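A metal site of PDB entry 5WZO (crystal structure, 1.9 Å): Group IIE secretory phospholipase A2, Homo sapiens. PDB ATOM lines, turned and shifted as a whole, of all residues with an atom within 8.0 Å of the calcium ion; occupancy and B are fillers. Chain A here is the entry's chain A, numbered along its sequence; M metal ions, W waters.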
ATOM      1  N   ASN A  21      10.881  14.798  20.138  1.00  0.00           N
ATOM      2  CA  ASN A  21      11.359  14.876  18.775  1.00  0.00           C
ATOM      3  C   ASN A  21      12.650  14.085  18.566  1.00  0.00           C
ATOM      4  O   ASN A  21      13.151  14.043  17.436  1.00  0.00           O
ATOM      5  CB  ASN A  21      11.456  16.319  18.244  1.00  0.00           C
ATOM      6  CG  ASN A  21      12.512  17.153  18.956  1.00  0.00           C
ATOM      7  OD1 ASN A  21      13.094  16.737  19.987  1.00  0.00           O
ATOM      8  ND2 ASN A  21      12.777  18.343  18.414  1.00  0.00           N
ATOM      9  N   TYR A  23      13.232  10.708  20.485  1.00  0.00           N
ATOM     10  CA  TYR A  23      12.989   9.616  21.421  1.00  0.00           C
ATOM     11  C   TYR A  23      13.020   8.272  20.732  1.00  0.00           C
ATOM     12  O   TYR A  23      12.518   8.153  19.616  1.00  0.00           O
ATOM     13  CB  TYR A  23      11.628   9.845  22.018  1.00  0.00           C
ATOM     14  CG  TYR A  23      11.140   8.879  23.102  1.00  0.00           C
ATOM     15  CD1 TYR A  23      10.548   7.641  22.768  1.00  0.00           C
ATOM     16  CD2 TYR A  23      11.197   9.258  24.449  1.00  0.00           C
ATOM     17  CE1 TYR A  23      10.061   6.797  23.744  1.00  0.00           C
ATOM     18  CE2 TYR A  23      10.725   8.413  25.443  1.00  0.00           C
ATOM     19  CZ  TYR A  23      10.139   7.188  25.091  1.00  0.00           C
ATOM     20  OH  TYR A  23       9.625   6.359  26.092  1.00  0.00           O
ATOM     21  N   CYS A  25      13.811   4.889  18.636  1.00  0.00           N
ATOM     22  CA  CYS A  25      14.376   4.603  17.337  1.00  0.00           C
ATOM     23  C   CYS A  25      13.630   5.312  16.212  1.00  0.00           C
ATOM     24  O   CYS A  25      14.164   5.397  15.108  1.00  0.00           O
ATOM     25  CB  CYS A  25      14.429   3.081  17.117  1.00  0.00           C
ATOM     26  SG  CYS A  25      15.581   2.341  18.334  1.00  0.00           S
ATOM     27  N   TYR A  26      12.411   5.804  16.494  1.00  0.00           N
ATOM     28  CA  TYR A  26      11.549   6.423  15.457  1.00  0.00           C
ATOM     29  C   TYR A  26      11.184   7.898  15.627  1.00  0.00           C
ATOM     30  O   TYR A  26      10.839   8.555  14.634  1.00  0.00           O
ATOM     31  CB  TYR A  26      10.266   5.581  15.248  1.00  0.00           C
ATOM     32  CG  TYR A  26      10.583   4.330  14.501  1.00  0.00           C
ATOM     33  CD1 TYR A  26      11.049   3.197  15.174  1.00  0.00           C
ATOM     34  CD2 TYR A  26      10.538   4.300  13.081  1.00  0.00           C
ATOM     35  CE1 TYR A  26      11.443   2.056  14.479  1.00  0.00           C
ATOM     36  CE2 TYR A  26      10.924   3.164  12.375  1.00  0.00           C
ATOM     37  CZ  TYR A  26      11.391   2.054  13.082  1.00  0.00           C
ATOM     38  OH  TYR A  26      11.744   0.896  12.434  1.00  0.00           O
ATOM     39  N   CYS A  27      11.213   8.422  16.851  1.00  0.00           N
ATOM     40  CA  CYS A  27      10.779   9.822  17.056  1.00  0.00           C
ATOM     41  C   CYS A  27      11.946  10.724  16.679  1.00  0.00           C
ATOM     42  O   CYS A  27      12.976  10.702  17.321  1.00  0.00           O
ATOM     43  CB  CYS A  27      10.324  10.087  18.478  1.00  0.00           C
ATOM     44  SG  CYS A  27       9.085   8.965  19.157  1.00  0.00           S
ATOM     45  N   GLY A  28      11.760  11.544  15.651  1.00  0.00           N
ATOM     46  CA  GLY A  28      12.933  12.218  15.062  1.00  0.00           C
ATOM     47  C   GLY A  28      13.143  11.806  13.632  1.00  0.00           C
ATOM     48  O   GLY A  28      12.352  11.026  13.093  1.00  0.00           O
ATOM     49  N   ILE A  29      14.184  12.303  12.984  1.00  0.00           N
ATOM     50  CA  ILE A  29      14.254  12.096  11.528  1.00  0.00           C
ATOM     51  C   ILE A  29      14.578  10.645  11.146  1.00  0.00           C
ATOM     52  O   ILE A  29      15.443   9.995  11.760  1.00  0.00           O
ATOM     53  CB  ILE A  29      15.111  13.180  10.794  1.00  0.00           C
ATOM     54  CG1 ILE A  29      16.594  13.047  11.120  1.00  0.00           C
ATOM     55  CG2 ILE A  29      14.587  14.597  11.083  1.00  0.00           C
ATOM     56  CD1 ILE A  29      17.379  12.315  10.042  1.00  0.00           C
ATOM     57  N   GLY A  30      13.848  10.110  10.178  1.00  0.00           N
ATOM     58  CA  GLY A  30      13.960   8.686   9.831  1.00  0.00           C
ATOM     59  C   GLY A  30      13.579   7.750  10.970  1.00  0.00           C
ATOM     60  O   GLY A  30      12.768   8.078  11.826  1.00  0.00           O
ATOM     61  N   GLY A  31      14.184   6.577  11.003  1.00  0.00           N
ATOM     62  CA  GLY A  31      13.734   5.527  11.870  1.00  0.00           C
ATOM     63  C   GLY A  31      14.083   4.209  11.219  1.00  0.00           C
ATOM     64  O   GLY A  31      14.011   4.080  10.028  1.00  0.00           O
ATOM     65  N   SER A  32      14.472   3.239  12.030  1.00  0.00           N
ATOM     66  CA  SER A  32      14.869   1.893  11.567  1.00  0.00           C
ATOM     67  C   SER A  32      14.858   0.978  12.807  1.00  0.00           C
ATOM     68  O   SER A  32      14.816   1.453  13.962  1.00  0.00           O
ATOM     69  CB  SER A  32      16.290   1.954  11.038  1.00  0.00           C
ATOM     70  OG  SER A  32      17.142   2.462  12.066  1.00  0.00           O
ATOM     71  N   ASP A  40       7.480   5.007  21.130  1.00  0.00           N
ATOM     72  CA  ASP A  40       8.228   4.830  19.875  1.00  0.00           C
ATOM     73  C   ASP A  40       7.338   4.303  18.767  1.00  0.00           C
ATOM     74  O   ASP A  40       7.490   4.720  17.622  1.00  0.00           O
ATOM     75  CB  ASP A  40       9.449   3.906  20.098  1.00  0.00           C
ATOM     76  CG  ASP A  40      10.628   4.248  19.230  1.00  0.00           C
ATOM     77  OD1 ASP A  40      10.609   5.328  18.578  1.00  0.00           O
ATOM     78  OD2 ASP A  40      11.642   3.447  19.218  1.00  0.00           O
ATOM     79  N   CYS A  43       5.597   6.841  16.994  1.00  0.00           N
ATOM     80  CA  CYS A  43       6.425   7.521  15.987  1.00  0.00           C
ATOM     81  C   CYS A  43       6.664   6.672  14.731  1.00  0.00           C
ATOM     82  O   CYS A  43       6.714   7.226  13.615  1.00  0.00           O
ATOM     83  CB  CYS A  43       7.784   7.931  16.571  1.00  0.00           C
ATOM     84  SG  CYS A  43       7.566   9.197  17.835  1.00  0.00           S
ATOM     85  N   HIS A  44       6.844   5.353  14.910  1.00  0.00           N
ATOM     86  CA  HIS A  44       6.832   4.431  13.758  1.00  0.00           C
ATOM     87  C   HIS A  44       5.552   4.642  12.891  1.00  0.00           C
ATOM     88  O   HIS A  44       5.628   4.834  11.668  1.00  0.00           O
ATOM     89  CB  HIS A  44       6.918   2.976  14.243  1.00  0.00           C
ATOM     90  CG  HIS A  44       6.879   1.972  13.113  1.00  0.00           C
ATOM     91  ND1 HIS A  44       5.694   1.465  12.608  1.00  0.00           N
ATOM     92  CD2 HIS A  44       7.876   1.420  12.397  1.00  0.00           C
ATOM     93  CE1 HIS A  44       5.975   0.623  11.629  1.00  0.00           C
ATOM     94  NE2 HIS A  44       7.296   0.559  11.493  1.00  0.00           N
ATOM     95  N   HIS A  46       3.466   7.292  12.863  1.00  0.00           N
ATOM     96  CA  HIS A  46       3.487   8.672  12.367  1.00  0.00           C
ATOM     97  C   HIS A  46       4.378   8.804  11.132  1.00  0.00           C
ATOM     98  O   HIS A  46       4.006   9.427  10.145  1.00  0.00           O
ATOM     99  CB  HIS A  46       4.008   9.597  13.477  1.00  0.00           C
ATOM    100  CG  HIS A  46       3.905  11.052  13.154  1.00  0.00           C
ATOM    101  ND1 HIS A  46       5.014  11.832  12.886  1.00  0.00           N
ATOM    102  CD2 HIS A  46       2.831  11.862  13.039  1.00  0.00           C
ATOM    103  CE1 HIS A  46       4.614  13.071  12.636  1.00  0.00           C
ATOM    104  NE2 HIS A  46       3.300  13.116  12.742  1.00  0.00           N
ATOM    105  N   ASP A  47       5.566   8.197  11.184  1.00  0.00           N
ATOM    106  CA  ASP A  47       6.428   8.135  10.021  1.00  0.00           C
ATOM    107  C   ASP A  47       5.693   7.498   8.814  1.00  0.00           C
ATOM    108  O   ASP A  47       5.822   7.984   7.683  1.00  0.00           O
ATOM    109  CB  ASP A  47       7.637   7.273  10.373  1.00  0.00           C
ATOM    110  CG  ASP A  47       8.704   8.019  11.169  1.00  0.00           C
ATOM    111  OD1 ASP A  47       8.492   9.199  11.570  1.00  0.00           O
ATOM    112  OD2 ASP A  47       9.783   7.416  11.374  1.00  0.00           O
ATOM    113  N   CYS A  48       4.973   6.392   9.058  1.00  0.00           N
ATOM    114  CA  CYS A  48       4.202   5.701   8.024  1.00  0.00           C
ATOM    115  C   CYS A  48       3.108   6.614   7.508  1.00  0.00           C
ATOM    116  O   CYS A  48       2.806   6.636   6.304  1.00  0.00           O
ATOM    117  CB  CYS A  48       3.515   4.445   8.616  1.00  0.00           C
ATOM    118  SG  CYS A  48       4.713   3.153   9.010  1.00  0.00           S
HETATM  119 CA    CA M   1      10.870   9.336  12.461  1.00  0.00          CA
HETATM  120  O   HOH W   1       9.690  11.399  13.585  1.00  0.00           O
HETATM  121  O   HOH W   2      10.789  10.487  10.109  1.00  0.00           O
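The backbone carbonyl oxygen (O) of Ser 32 lies close to the side-chain hydroxyl (OH) of Tyr 26 (3.5 Å). The backbone NH of Tyr 26 sits at hydrogen-bond distance from the side-chain carboxylate of Asp 40, 2.8 Å away. O of Asn 21 sits close to N of Gly 28. SG of Cys 27 is disulfide-bonded to SG of Cys 43, at 2.0 Å.
Within 4 Å of the calcium ion: Tyr 26, Gly 28, Gly 30 and Asp 47. Along chain A the residues within 4 Å of the calcium ion span positions 26 to 47.
O of Tyr 26 binds the calcium ion, at 2.3 Å. O of Gly 28 is bound to the calcium ion, at 2.3 Å. The calcium ion is bound by the backbone carbonyl oxygen (O) of Gly 30 (2.4 Å). The calcium ion is bound by OD2 of Asp 47, at 2.5 Å. OD1 of Asp 47 is bound to the calcium ion, 2.5 Å away. Water W2 binds the calcium ion (2.6 Å). Water W1 is bound to the calcium ion (2.6 Å).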
